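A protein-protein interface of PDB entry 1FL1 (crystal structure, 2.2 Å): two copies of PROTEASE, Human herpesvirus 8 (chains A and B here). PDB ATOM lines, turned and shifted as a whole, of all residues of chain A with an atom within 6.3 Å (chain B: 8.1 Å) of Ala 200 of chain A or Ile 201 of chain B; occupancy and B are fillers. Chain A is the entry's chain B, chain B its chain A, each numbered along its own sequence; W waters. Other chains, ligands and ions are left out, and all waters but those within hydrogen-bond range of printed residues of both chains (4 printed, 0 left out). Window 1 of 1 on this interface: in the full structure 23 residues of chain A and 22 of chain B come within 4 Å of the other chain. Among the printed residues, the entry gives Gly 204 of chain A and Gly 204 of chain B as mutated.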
ATOM      1  N   GLU A  45      11.120   3.451   7.281  1.00  0.00           N
ATOM      2  CA  GLU A  45       9.943   4.283   7.477  1.00  0.00           C
ATOM      3  C   GLU A  45      10.276   5.640   8.089  1.00  0.00           C
ATOM      4  O   GLU A  45       9.530   6.156   8.925  1.00  0.00           O
ATOM      5  CB  GLU A  45       8.931   3.547   8.361  1.00  0.00           C
ATOM      6  CG  GLU A  45       8.419   2.211   7.812  1.00  0.00           C
ATOM      7  CD  GLU A  45       7.335   2.356   6.747  1.00  0.00           C
ATOM      8  OE1 GLU A  45       6.637   1.355   6.466  1.00  0.00           O
ATOM      9  OE2 GLU A  45       7.171   3.457   6.183  1.00  0.00           O
ATOM     10  N   LEU A  83      12.957 -12.801  11.597  1.00  0.00           N
ATOM     11  CA  LEU A  83      11.627 -12.613  11.037  1.00  0.00           C
ATOM     12  C   LEU A  83      11.327 -13.646   9.961  1.00  0.00           C
ATOM     13  O   LEU A  83      10.289 -14.298   9.993  1.00  0.00           O
ATOM     14  CB  LEU A  83      11.497 -11.215  10.445  1.00  0.00           C
ATOM     15  CG  LEU A  83      10.814 -10.104  11.248  1.00  0.00           C
ATOM     16  CD1 LEU A  83      10.785 -10.418  12.741  1.00  0.00           C
ATOM     17  CD2 LEU A  83      11.548  -8.788  10.956  1.00  0.00           C
ATOM     18  N   SER A  87       8.235 -16.318   9.471  1.00  0.00           N
ATOM     19  CA  SER A  87       7.329 -15.802   8.459  1.00  0.00           C
ATOM     20  C   SER A  87       6.877 -16.883   7.491  1.00  0.00           C
ATOM     21  O   SER A  87       7.535 -17.907   7.313  1.00  0.00           O
ATOM     22  CB  SER A  87       7.995 -14.681   7.663  1.00  0.00           C
ATOM     23  OG  SER A  87       7.221 -14.360   6.513  1.00  0.00           O
ATOM     24  N   ILE A 105      11.597 -11.867   2.880  1.00  0.00           N
ATOM     25  CA  ILE A 105      10.958 -11.186   3.996  1.00  0.00           C
ATOM     26  C   ILE A 105      11.073  -9.682   3.747  1.00  0.00           C
ATOM     27  O   ILE A 105      10.142  -8.928   4.038  1.00  0.00           O
ATOM     28  CB  ILE A 105      11.604 -11.568   5.369  1.00  0.00           C
ATOM     29  CG1 ILE A 105      10.758 -11.022   6.526  1.00  0.00           C
ATOM     30  CG2 ILE A 105      12.982 -10.966   5.498  1.00  0.00           C
ATOM     31  CD1 ILE A 105       9.377 -11.627   6.627  1.00  0.00           C
ATOM     32  N   THR A 108       8.416  -8.497   1.576  1.00  0.00           N
ATOM     33  CA  THR A 108       7.078  -8.583   2.159  1.00  0.00           C
ATOM     34  C   THR A 108       6.880  -7.417   3.116  1.00  0.00           C
ATOM     35  O   THR A 108       5.811  -6.789   3.177  1.00  0.00           O
ATOM     36  CB  THR A 108       6.904  -9.891   2.960  1.00  0.00           C
ATOM     37  OG1 THR A 108       7.103 -11.015   2.094  1.00  0.00           O
ATOM     38  CG2 THR A 108       5.507  -9.969   3.553  1.00  0.00           C
ATOM     39  N   TRP A 109       7.956  -7.131   3.836  1.00  0.00           N
ATOM     40  CA  TRP A 109       8.014  -6.097   4.851  1.00  0.00           C
ATOM     41  C   TRP A 109       8.276  -4.679   4.348  1.00  0.00           C
ATOM     42  O   TRP A 109       7.456  -3.778   4.568  1.00  0.00           O
ATOM     43  CB  TRP A 109       9.074  -6.523   5.871  1.00  0.00           C
ATOM     44  CG  TRP A 109       9.335  -5.602   7.019  1.00  0.00           C
ATOM     45  CD1 TRP A 109       8.525  -4.603   7.484  1.00  0.00           C
ATOM     46  CD2 TRP A 109      10.472  -5.636   7.891  1.00  0.00           C
ATOM     47  NE1 TRP A 109       9.086  -4.017   8.592  1.00  0.00           N
ATOM     48  CE2 TRP A 109      10.279  -4.635   8.872  1.00  0.00           C
ATOM     49  CE3 TRP A 109      11.631  -6.424   7.949  1.00  0.00           C
ATOM     50  CZ2 TRP A 109      11.209  -4.384   9.891  1.00  0.00           C
ATOM     51  CZ3 TRP A 109      12.562  -6.178   8.969  1.00  0.00           C
ATOM     52  CH2 TRP A 109      12.336  -5.169   9.928  1.00  0.00           C
ATOM     53  N   LEU A 110       9.400  -4.476   3.660  1.00  0.00           N
ATOM     54  CA  LEU A 110       9.757  -3.144   3.180  1.00  0.00           C
ATOM     55  C   LEU A 110      10.043  -3.098   1.681  1.00  0.00           C
ATOM     56  O   LEU A 110      11.176  -2.862   1.253  1.00  0.00           O
ATOM     57  CB  LEU A 110      10.970  -2.651   3.961  1.00  0.00           C
ATOM     58  CG  LEU A 110      10.781  -2.652   5.481  1.00  0.00           C
ATOM     59  CD1 LEU A 110      12.143  -2.683   6.157  1.00  0.00           C
ATOM     60  CD2 LEU A 110       9.957  -1.435   5.920  1.00  0.00           C
ATOM     61  N   THR A 195       8.216  -0.098  17.797  1.00  0.00           N
ATOM     62  CA  THR A 195       8.042   0.990  16.838  1.00  0.00           C
ATOM     63  C   THR A 195       7.961   0.493  15.388  1.00  0.00           C
ATOM     64  O   THR A 195       7.176   1.010  14.588  1.00  0.00           O
ATOM     65  CB  THR A 195       9.194   1.990  16.966  1.00  0.00           C
ATOM     66  OG1 THR A 195       9.366   2.318  18.349  1.00  0.00           O
ATOM     67  CG2 THR A 195       8.891   3.266  16.187  1.00  0.00           C
ATOM     68  N   LEU A 196       8.773  -0.508  15.057  1.00  0.00           N
ATOM     69  CA  LEU A 196       8.789  -1.072  13.709  1.00  0.00           C
ATOM     70  C   LEU A 196       7.532  -1.917  13.529  1.00  0.00           C
ATOM     71  O   LEU A 196       6.860  -1.867  12.490  1.00  0.00           O
ATOM     72  CB  LEU A 196      10.052  -1.930  13.506  1.00  0.00           C
ATOM     73  CG  LEU A 196      11.385  -1.160  13.543  1.00  0.00           C
ATOM     74  CD1 LEU A 196      12.550  -2.124  13.682  1.00  0.00           C
ATOM     75  CD2 LEU A 196      11.526  -0.317  12.280  1.00  0.00           C
ATOM     76  N   MET A 197       7.208  -2.692  14.557  1.00  0.00           N
ATOM     77  CA  MET A 197       6.023  -3.525  14.504  1.00  0.00           C
ATOM     78  C   MET A 197       4.761  -2.695  14.266  1.00  0.00           C
ATOM     79  O   MET A 197       3.900  -3.086  13.475  1.00  0.00           O
ATOM     80  CB  MET A 197       5.885  -4.325  15.784  1.00  0.00           C
ATOM     81  CG  MET A 197       4.833  -5.397  15.684  1.00  0.00           C
ATOM     82  SD  MET A 197       4.913  -6.473  17.087  1.00  0.00           S
ATOM     83  CE  MET A 197       3.490  -7.532  16.784  1.00  0.00           C
ATOM     84  N   ALA A 198       4.653  -1.549  14.934  1.00  0.00           N
ATOM     85  CA  ALA A 198       3.489  -0.686  14.755  1.00  0.00           C
ATOM     86  C   ALA A 198       3.374  -0.269  13.286  1.00  0.00           C
ATOM     87  O   ALA A 198       2.277  -0.252  12.720  1.00  0.00           O
ATOM     88  CB  ALA A 198       3.599   0.547  15.660  1.00  0.00           C
ATOM     89  N   LYS A 199       4.502   0.076  12.666  1.00  0.00           N
ATOM     90  CA  LYS A 199       4.496   0.449  11.249  1.00  0.00           C
ATOM     91  C   LYS A 199       4.056  -0.738  10.394  1.00  0.00           C
ATOM     92  O   LYS A 199       3.326  -0.581   9.424  1.00  0.00           O
ATOM     93  CB  LYS A 199       5.888   0.889  10.804  1.00  0.00           C
ATOM     94  CG  LYS A 199       6.283   2.250  11.303  1.00  0.00           C
ATOM     95  CD  LYS A 199       5.430   3.323  10.662  1.00  0.00           C
ATOM     96  CE  LYS A 199       5.905   4.698  11.101  1.00  0.00           C
ATOM     97  NZ  LYS A 199       5.047   5.781  10.550  1.00  0.00           N
ATOM     98  N   ALA A 200       4.517  -1.929  10.756  1.00  0.00           N
ATOM     99  CA  ALA A 200       4.162  -3.135  10.021  1.00  0.00           C
ATOM    100  C   ALA A 200       2.651  -3.357  10.130  1.00  0.00           C
ATOM    101  O   ALA A 200       1.988  -3.683   9.144  1.00  0.00           O
ATOM    102  CB  ALA A 200       4.929  -4.343  10.589  1.00  0.00           C
ATOM    103  N   ILE A 201       2.112  -3.181  11.336  1.00  0.00           N
ATOM    104  CA  ILE A 201       0.673  -3.341  11.556  1.00  0.00           C
ATOM    105  C   ILE A 201      -0.090  -2.315  10.721  1.00  0.00           C
ATOM    106  O   ILE A 201      -1.036  -2.667  10.012  1.00  0.00           O
ATOM    107  CB  ILE A 201       0.313  -3.137  13.041  1.00  0.00           C
ATOM    108  CG1 ILE A 201       0.923  -4.260  13.873  1.00  0.00           C
ATOM    109  CG2 ILE A 201      -1.204  -3.051  13.210  1.00  0.00           C
ATOM    110  CD1 ILE A 201       0.838  -4.034  15.362  1.00  0.00           C
ATOM    111  N   ASP A 202       0.319  -1.048  10.798  1.00  0.00           N
ATOM    112  CA  ASP A 202      -0.351   0.008  10.034  1.00  0.00           C
ATOM    113  C   ASP A 202      -0.328  -0.258   8.529  1.00  0.00           C
ATOM    114  O   ASP A 202      -1.257   0.116   7.812  1.00  0.00           O
ATOM    115  CB  ASP A 202       0.295   1.384  10.285  1.00  0.00           C
ATOM    116  CG  ASP A 202       0.128   1.875  11.724  1.00  0.00           C
ATOM    117  OD1 ASP A 202      -0.779   1.375  12.434  1.00  0.00           O
ATOM    118  OD2 ASP A 202       0.899   2.776  12.140  1.00  0.00           O
ATOM    119  N   ALA A 203       0.732  -0.900   8.048  1.00  0.00           N
ATOM    120  CA  ALA A 203       0.861  -1.171   6.622  1.00  0.00           C
ATOM    121  C   ALA A 203      -0.253  -2.049   6.058  1.00  0.00           C
ATOM    122  O   ALA A 203      -0.734  -1.801   4.956  1.00  0.00           O
ATOM    123  CB  ALA A 203       2.239  -1.799   6.326  1.00  0.00           C
ATOM    124  N   GLY A 204      -0.651  -3.078   6.799  1.00  0.00           N
ATOM    125  CA  GLY A 204      -1.708  -3.956   6.322  1.00  0.00           C
ATOM    126  C   GLY A 204      -3.023  -3.220   6.111  1.00  0.00           C
ATOM    127  O   GLY A 204      -3.941  -3.730   5.467  1.00  0.00           O
ATOM    128  N   PHE A 205      -3.132  -2.010   6.650  1.00  0.00           N
ATOM    129  CA  PHE A 205      -4.363  -1.262   6.477  1.00  0.00           C
ATOM    130  C   PHE A 205      -4.253  -0.131   5.485  1.00  0.00           C
ATOM    131  O   PHE A 205      -5.171   0.677   5.353  1.00  0.00           O
ATOM    132  CB  PHE A 205      -4.886  -0.770   7.827  1.00  0.00           C
ATOM    133  CG  PHE A 205      -5.875  -1.707   8.439  1.00  0.00           C
ATOM    134  CD1 PHE A 205      -7.239  -1.535   8.227  1.00  0.00           C
ATOM    135  CD2 PHE A 205      -5.442  -2.821   9.145  1.00  0.00           C
ATOM    136  CE1 PHE A 205      -8.155  -2.469   8.703  1.00  0.00           C
ATOM    137  CE2 PHE A 205      -6.353  -3.762   9.624  1.00  0.00           C
ATOM    138  CZ  PHE A 205      -7.710  -3.586   9.402  1.00  0.00           C
ATOM    139  N   ARG A 209      -2.663  -1.334  -1.081  1.00  0.00           N
ATOM    140  CA  ARG A 209      -1.215  -1.489  -1.030  1.00  0.00           C
ATOM    141  C   ARG A 209      -0.730  -2.569  -1.992  1.00  0.00           C
ATOM    142  O   ARG A 209       0.212  -2.352  -2.754  1.00  0.00           O
ATOM    143  CB  ARG A 209      -0.766  -1.836   0.390  1.00  0.00           C
ATOM    144  CG  ARG A 209       0.732  -2.066   0.517  1.00  0.00           C
ATOM    145  CD  ARG A 209       1.152  -2.191   1.971  1.00  0.00           C
ATOM    146  NE  ARG A 209       2.563  -2.543   2.099  1.00  0.00           N
ATOM    147  CZ  ARG A 209       3.009  -3.662   2.662  1.00  0.00           C
ATOM    148  NH1 ARG A 209       2.154  -4.545   3.160  1.00  0.00           N
ATOM    149  NH2 ARG A 209       4.315  -3.903   2.726  1.00  0.00           N
ATOM    150  N   GLU B  45      -2.864 -15.713  16.861  1.00  0.00           N
ATOM    151  CA  GLU B  45      -2.538 -16.445  15.643  1.00  0.00           C
ATOM    152  C   GLU B  45      -2.156 -17.907  15.877  1.00  0.00           C
ATOM    153  O   GLU B  45      -1.290 -18.446  15.191  1.00  0.00           O
ATOM    154  CB  GLU B  45      -1.400 -15.716  14.906  1.00  0.00           C
ATOM    155  CG  GLU B  45      -1.732 -14.272  14.473  1.00  0.00           C
ATOM    156  CD  GLU B  45      -2.415 -14.192  13.116  1.00  0.00           C
ATOM    157  OE1 GLU B  45      -2.888 -15.232  12.612  1.00  0.00           O
ATOM    158  OE2 GLU B  45      -2.491 -13.083  12.548  1.00  0.00           O
ATOM    159  N   LEU B  83       2.305  -0.334  21.282  1.00  0.00           N
ATOM    160  CA  LEU B  83       2.096  -0.292  19.834  1.00  0.00           C
ATOM    161  C   LEU B  83       1.160   0.832  19.417  1.00  0.00           C
ATOM    162  O   LEU B  83       1.391   1.503  18.408  1.00  0.00           O
ATOM    163  CB  LEU B  83       1.528  -1.617  19.325  1.00  0.00           C
ATOM    164  CG  LEU B  83       2.461  -2.827  19.359  1.00  0.00           C
ATOM    165  CD1 LEU B  83       1.680  -4.089  18.988  1.00  0.00           C
ATOM    166  CD2 LEU B  83       3.630  -2.600  18.398  1.00  0.00           C
ATOM    167  N   THR B 108      -6.752  -3.086  14.355  1.00  0.00           N
ATOM    168  CA  THR B 108      -5.899  -2.935  13.179  1.00  0.00           C
ATOM    169  C   THR B 108      -4.987  -4.157  13.059  1.00  0.00           C
ATOM    170  O   THR B 108      -4.724  -4.661  11.968  1.00  0.00           O
ATOM    171  CB  THR B 108      -5.005  -1.668  13.287  1.00  0.00           C
ATOM    172  OG1 THR B 108      -5.829  -0.511  13.491  1.00  0.00           O
ATOM    173  CG2 THR B 108      -4.185  -1.480  12.002  1.00  0.00           C
ATOM    174  N   TRP B 109      -4.540  -4.627  14.214  1.00  0.00           N
ATOM    175  CA  TRP B 109      -3.632  -5.745  14.340  1.00  0.00           C
ATOM    176  C   TRP B 109      -4.307  -7.125  14.332  1.00  0.00           C
ATOM    177  O   TRP B 109      -3.965  -8.001  13.513  1.00  0.00           O
ATOM    178  CB  TRP B 109      -2.822  -5.506  15.629  1.00  0.00           C
ATOM    179  CG  TRP B 109      -1.794  -6.511  15.977  1.00  0.00           C
ATOM    180  CD1 TRP B 109      -1.193  -7.394  15.133  1.00  0.00           C
ATOM    181  CD2 TRP B 109      -1.244  -6.758  17.279  1.00  0.00           C
ATOM    182  NE1 TRP B 109      -0.310  -8.185  15.827  1.00  0.00           N
ATOM    183  CE2 TRP B 109      -0.323  -7.822  17.145  1.00  0.00           C
ATOM    184  CE3 TRP B 109      -1.450  -6.196  18.548  1.00  0.00           C
ATOM    185  CZ2 TRP B 109       0.403  -8.331  18.231  1.00  0.00           C
ATOM    186  CZ3 TRP B 109      -0.725  -6.706  19.636  1.00  0.00           C
ATOM    187  CH2 TRP B 109       0.185  -7.768  19.465  1.00  0.00           C
ATOM    188  N   ALA B 139      -5.179 -11.961  12.319  1.00  0.00           N
ATOM    189  CA  ALA B 139      -5.164 -10.876  11.346  1.00  0.00           C
ATOM    190  C   ALA B 139      -6.447 -10.992  10.514  1.00  0.00           C
ATOM    191  O   ALA B 139      -6.967 -10.001  10.015  1.00  0.00           O
ATOM    192  CB  ALA B 139      -3.943 -11.001  10.445  1.00  0.00           C
ATOM    193  N   GLU B 194       9.537 -11.003  18.025  1.00  0.00           N
ATOM    194  CA  GLU B 194       9.835 -11.309  16.629  1.00  0.00           C
ATOM    195  C   GLU B 194       8.747 -12.146  15.977  1.00  0.00           C
ATOM    196  O   GLU B 194       8.271 -11.830  14.887  1.00  0.00           O
ATOM    197  CB  GLU B 194      11.171 -12.059  16.508  1.00  0.00           C
ATOM    198  CG  GLU B 194      12.421 -11.193  16.556  1.00  0.00           C
ATOM    199  CD  GLU B 194      12.673 -10.597  17.923  1.00  0.00           C
ATOM    200  OE1 GLU B 194      12.157 -11.147  18.926  1.00  0.00           O
ATOM    201  OE2 GLU B 194      13.405  -9.584  17.997  1.00  0.00           O
ATOM    202  N   THR B 195       8.362 -13.216  16.657  1.00  0.00           N
ATOM    203  CA  THR B 195       7.349 -14.129  16.161  1.00  0.00           C
ATOM    204  C   THR B 195       6.023 -13.430  15.854  1.00  0.00           C
ATOM    205  O   THR B 195       5.378 -13.722  14.844  1.00  0.00           O
ATOM    206  CB  THR B 195       7.125 -15.254  17.184  1.00  0.00           C
ATOM    207  OG1 THR B 195       8.386 -15.846  17.509  1.00  0.00           O
ATOM    208  CG2 THR B 195       6.216 -16.329  16.616  1.00  0.00           C
ATOM    209  N   LEU B 196       5.619 -12.508  16.723  1.00  0.00           N
ATOM    210  CA  LEU B 196       4.368 -11.782  16.522  1.00  0.00           C
ATOM    211  C   LEU B 196       4.522 -10.809  15.362  1.00  0.00           C
ATOM    212  O   LEU B 196       3.622 -10.653  14.539  1.00  0.00           O
ATOM    213  CB  LEU B 196       3.970 -11.030  17.804  1.00  0.00           C
ATOM    214  CG  LEU B 196       3.583 -11.897  19.015  1.00  0.00           C
ATOM    215  CD1 LEU B 196       3.280 -11.011  20.222  1.00  0.00           C
ATOM    216  CD2 LEU B 196       2.365 -12.737  18.675  1.00  0.00           C
ATOM    217  N   MET B 197       5.676 -10.157  15.288  1.00  0.00           N
ATOM    218  CA  MET B 197       5.914  -9.220  14.205  1.00  0.00           C
ATOM    219  C   MET B 197       5.896  -9.930  12.846  1.00  0.00           C
ATOM    220  O   MET B 197       5.352  -9.403  11.874  1.00  0.00           O
ATOM    221  CB  MET B 197       7.242  -8.505  14.406  1.00  0.00           C
ATOM    222  CG  MET B 197       7.465  -7.410  13.391  1.00  0.00           C
ATOM    223  SD  MET B 197       8.845  -6.380  13.813  1.00  0.00           S
ATOM    224  CE  MET B 197       8.857  -5.266  12.398  1.00  0.00           C
ATOM    225  N   ALA B 198       6.474 -11.128  12.779  1.00  0.00           N
ATOM    226  CA  ALA B 198       6.486 -11.869  11.520  1.00  0.00           C
ATOM    227  C   ALA B 198       5.044 -12.045  11.048  1.00  0.00           C
ATOM    228  O   ALA B 198       4.740 -11.859   9.866  1.00  0.00           O
ATOM    229  CB  ALA B 198       7.160 -13.234  11.704  1.00  0.00           C
ATOM    230  N   LYS B 199       4.159 -12.394  11.981  1.00  0.00           N
ATOM    231  CA  LYS B 199       2.738 -12.588  11.673  1.00  0.00           C
ATOM    232  C   LYS B 199       2.090 -11.310  11.162  1.00  0.00           C
ATOM    233  O   LYS B 199       1.287 -11.341  10.232  1.00  0.00           O
ATOM    234  CB  LYS B 199       1.975 -13.064  12.914  1.00  0.00           C
ATOM    235  CG  LYS B 199       2.208 -14.511  13.281  1.00  0.00           C
ATOM    236  CD  LYS B 199       1.659 -15.447  12.221  1.00  0.00           C
ATOM    237  CE  LYS B 199       1.766 -16.885  12.679  1.00  0.00           C
ATOM    238  NZ  LYS B 199       1.369 -17.797  11.571  1.00  0.00           N
ATOM    239  N   ALA B 200       2.430 -10.190  11.780  1.00  0.00           N
ATOM    240  CA  ALA B 200       1.883  -8.900  11.370  1.00  0.00           C
ATOM    241  C   ALA B 200       2.350  -8.541   9.958  1.00  0.00           C
ATOM    242  O   ALA B 200       1.594  -7.975   9.173  1.00  0.00           O
ATOM    243  CB  ALA B 200       2.309  -7.810  12.355  1.00  0.00           C
ATOM    244  N   ILE B 201       3.602  -8.857   9.639  1.00  0.00           N
ATOM    245  CA  ILE B 201       4.122  -8.558   8.307  1.00  0.00           C
ATOM    246  C   ILE B 201       3.407  -9.432   7.287  1.00  0.00           C
ATOM    247  O   ILE B 201       3.025  -8.957   6.225  1.00  0.00           O
ATOM    248  CB  ILE B 201       5.659  -8.793   8.225  1.00  0.00           C
ATOM    249  CG1 ILE B 201       6.380  -7.732   9.067  1.00  0.00           C
ATOM    250  CG2 ILE B 201       6.129  -8.740   6.767  1.00  0.00           C
ATOM    251  CD1 ILE B 201       7.847  -8.031   9.335  1.00  0.00           C
ATOM    252  N   ASP B 202       3.221 -10.708   7.619  1.00  0.00           N
ATOM    253  CA  ASP B 202       2.527 -11.635   6.731  1.00  0.00           C
ATOM    254  C   ASP B 202       1.082 -11.186   6.497  1.00  0.00           C
ATOM    255  O   ASP B 202       0.582 -11.262   5.383  1.00  0.00           O
ATOM    256  CB  ASP B 202       2.522 -13.054   7.320  1.00  0.00           C
ATOM    257  CG  ASP B 202       3.879 -13.739   7.243  1.00  0.00           C
ATOM    258  OD1 ASP B 202       4.056 -14.784   7.914  1.00  0.00           O
ATOM    259  OD2 ASP B 202       4.768 -13.244   6.516  1.00  0.00           O
ATOM    260  N   ALA B 203       0.407 -10.727   7.547  1.00  0.00           N
ATOM    261  CA  ALA B 203      -0.977 -10.284   7.406  1.00  0.00           C
ATOM    262  C   ALA B 203      -1.110  -9.284   6.269  1.00  0.00           C
ATOM    263  O   ALA B 203      -2.101  -9.291   5.535  1.00  0.00           O
ATOM    264  CB  ALA B 203      -1.463  -9.652   8.702  1.00  0.00           C
ATOM    265  N   GLY B 204      -0.106  -8.426   6.132  1.00  0.00           N
ATOM    266  CA  GLY B 204      -0.134  -7.417   5.095  1.00  0.00           C
ATOM    267  C   GLY B 204      -0.246  -7.998   3.701  1.00  0.00           C
ATOM    268  O   GLY B 204      -0.705  -7.326   2.778  1.00  0.00           O
ATOM    269  N   PHE B 205       0.168  -9.252   3.543  1.00  0.00           N
ATOM    270  CA  PHE B 205       0.107  -9.891   2.237  1.00  0.00           C
ATOM    271  C   PHE B 205      -1.000 -10.919   2.069  1.00  0.00           C
ATOM    272  O   PHE B 205      -0.962 -11.724   1.142  1.00  0.00           O
ATOM    273  CB  PHE B 205       1.473 -10.495   1.878  1.00  0.00           C
ATOM    274  CG  PHE B 205       2.372  -9.528   1.165  1.00  0.00           C
ATOM    275  CD1 PHE B 205       2.552  -9.611  -0.215  1.00  0.00           C
ATOM    276  CD2 PHE B 205       2.952  -8.470   1.853  1.00  0.00           C
ATOM    277  CE1 PHE B 205       3.294  -8.644  -0.899  1.00  0.00           C
ATOM    278  CE2 PHE B 205       3.693  -7.497   1.184  1.00  0.00           C
ATOM    279  CZ  PHE B 205       3.862  -7.582  -0.196  1.00  0.00           C
ATOM    280  N   ILE B 206      -1.983 -10.894   2.969  1.00  0.00           N
ATOM    281  CA  ILE B 206      -3.126 -11.798   2.860  1.00  0.00           C
ATOM    282  C   ILE B 206      -4.003 -11.130   1.820  1.00  0.00           C
ATOM    283  O   ILE B 206      -4.453 -10.002   2.012  1.00  0.00           O
ATOM    284  CB  ILE B 206      -3.916 -11.903   4.181  1.00  0.00           C
ATOM    285  CG1 ILE B 206      -3.029 -12.512   5.263  1.00  0.00           C
ATOM    286  CG2 ILE B 206      -5.177 -12.733   3.977  1.00  0.00           C
ATOM    287  CD1 ILE B 206      -3.656 -12.502   6.635  1.00  0.00           C
ATOM    288  N   ARG B 209      -7.709  -9.234   2.147  1.00  0.00           N
ATOM    289  CA  ARG B 209      -7.923  -9.148   3.586  1.00  0.00           C
ATOM    290  C   ARG B 209      -8.894  -8.047   3.990  1.00  0.00           C
ATOM    291  O   ARG B 209      -9.893  -8.309   4.661  1.00  0.00           O
ATOM    292  CB  ARG B 209      -6.599  -8.920   4.303  1.00  0.00           C
ATOM    293  CG  ARG B 209      -6.739  -8.949   5.804  1.00  0.00           C
ATOM    294  CD  ARG B 209      -5.445  -8.598   6.466  1.00  0.00           C
ATOM    295  NE  ARG B 209      -5.572  -8.575   7.917  1.00  0.00           N
ATOM    296  CZ  ARG B 209      -5.054  -7.624   8.680  1.00  0.00           C
ATOM    297  NH1 ARG B 209      -4.385  -6.622   8.119  1.00  0.00           N
ATOM    298  NH2 ARG B 209      -5.188  -7.678   9.997  1.00  0.00           N
HETATM  299  O   HOH W   1       3.444  -6.556   4.906  1.00  0.00           O
HETATM  300  O   HOH W   2      -2.626  -4.843   9.814  1.00  0.00           O
HETATM  301  O   HOH W   3      -0.648  -4.458   2.866  1.00  0.00           O
HETATM  302  O   HOH W   4      -3.836  -6.271   5.253  1.00  0.00           O
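Water W4 lies within hydrogen-bond range of O of Gly 204 of chain A, NH1 of Arg 209 of chain B and O of Ala 203 of chain B.
Water W2 lies within hydrogen-bond range of the backbone carbonyl oxygen of Ile 201 of chain A (2.7 Å), the backbone carbonyl oxygen of Thr 108 of chain B (3.0 Å) and the guanidinium group of Arg 209 of chain B (3.0 Å).
Water W1 lies within hydrogen-bond range of O of Ile 201 of chain B, O of Thr 108 of chain A and NH1 of Arg 209 of chain A.
Water W3 lies within hydrogen-bond range of NH1 of Arg 209 of chain A, O of Gly 204 of chain B and O of Ala 203 of chain A.
Hydrophobic or aromatic side chains of chain B that line the printed part of chain A: Leu 83, Trp 109, Leu 196, Met 197, Ala 198, Ile 201 and Phe 205.
Hydrophobic or aromatic side chains of chain A within 4 Å of the printed part of chain B: Leu 83, Trp 109, Leu 196, Met 197, Ala 198, Ala 200, Ile 201 and Phe 205.
Of the printed residues of chain B, Met 197 of chain A touches Leu 83, Trp 109, Leu 196 and Met 197.
Printed residues of chain B within 4 Å of Ala 198 of chain A: Leu 83 (3.7 Å).
Printed residues of chain B within 4 Å of Ala 200 of chain A: Ile 201 (3.99 Å).
Of the printed residues of chain A, Leu 196 of chain B touches Met 197.
Printed residues of chain A within 4 Å of Ile 201 of chain B: Thr 108 (3.5 Å), Trp 109 (3.7 Å) and Ala 200 (3.99 Å).
The nearest printed residue of chain B that does not touch Ala 200 of chain A is Ala 200 of chain B (4.3 Å).
Among the printed residues, pairs that only touch across the chains: Phe 205 of chain A with Thr 108 of chain B (3.0 Å), Thr 108 of chain A with Phe 205 of chain B (3.0 Å), Thr 108 of chain A with Ile 201 of chain B (3.5 Å), Met 197 of chain A with Trp 109 of chain B (3.5 Å), Trp 109 of chain A with Met 197 of chain B (3.5 Å), Ile 201 of chain A with Thr 108 of chain B (3.6 Å), Leu 83 of chain A with Glu 194 of chain B (3.6 Å), Ala 198 of chain A with Leu 83 of chain B (3.7 Å), Ile 201 of chain A with Trp 109 of chain B (3.7 Å), Trp 109 of chain A with Ile 201 of chain B (3.7 Å), Met 197 of chain A with Leu 196 of chain B (3.7 Å), Leu 196 of chain A with Met 197 of chain B (3.7 Å), Leu 83 of chain A with Ala 198 of chain B (3.7 Å), Ile 201 of chain A with Leu 83 of chain B (3.7 Å), Met 197 of chain A with Met 197 of chain B (3.7 Å), Phe 205 of chain A with Arg 209 of chain B (3.8 Å), Met 197 of chain A with Leu 83 of chain B (3.9 Å), Arg 209 of chain A with Phe 205 of chain B (3.9 Å), Gly 204 of chain A with Arg 209 of chain B (3.9 Å), Ser 87 of chain A with Ala 198 of chain B (3.96 Å), Ala 200 of chain A with Ile 201 of chain B (3.99 Å) and Gly 204 of chain A with Gly 204 of chain B (3.995 Å).
NE of Arg 209 of chain B is in hydrogen-bond range of O of Ala 139 of chain B (2.9 Å).
O of Thr 108 of chain A lies within hydrogen-bond range of NH2 of Arg 209 of chain A.
OG of Ser 87 of chain A sits at hydrogen-bond distance from OD2 of Asp 202 of chain B, 2.7 Å away.
Trp 109 of chain A touches Met 197 of chain B, and with the chains exchanged Met 197 of chain A touches Trp 109 of chain B.
Leu 196 of chain A touches Met 197 of chain B, and with the chains exchanged Met 197 of chain A touches Leu 196 of chain B.
Ile 201 of chain A touches Leu 83 of chain B, but with the chains exchanged Leu 83 of chain A does not touch Ile 201 of chain B (4.1 Å).
Gly 204 of chain A touches its own counterpart, Gly 204 of chain B.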
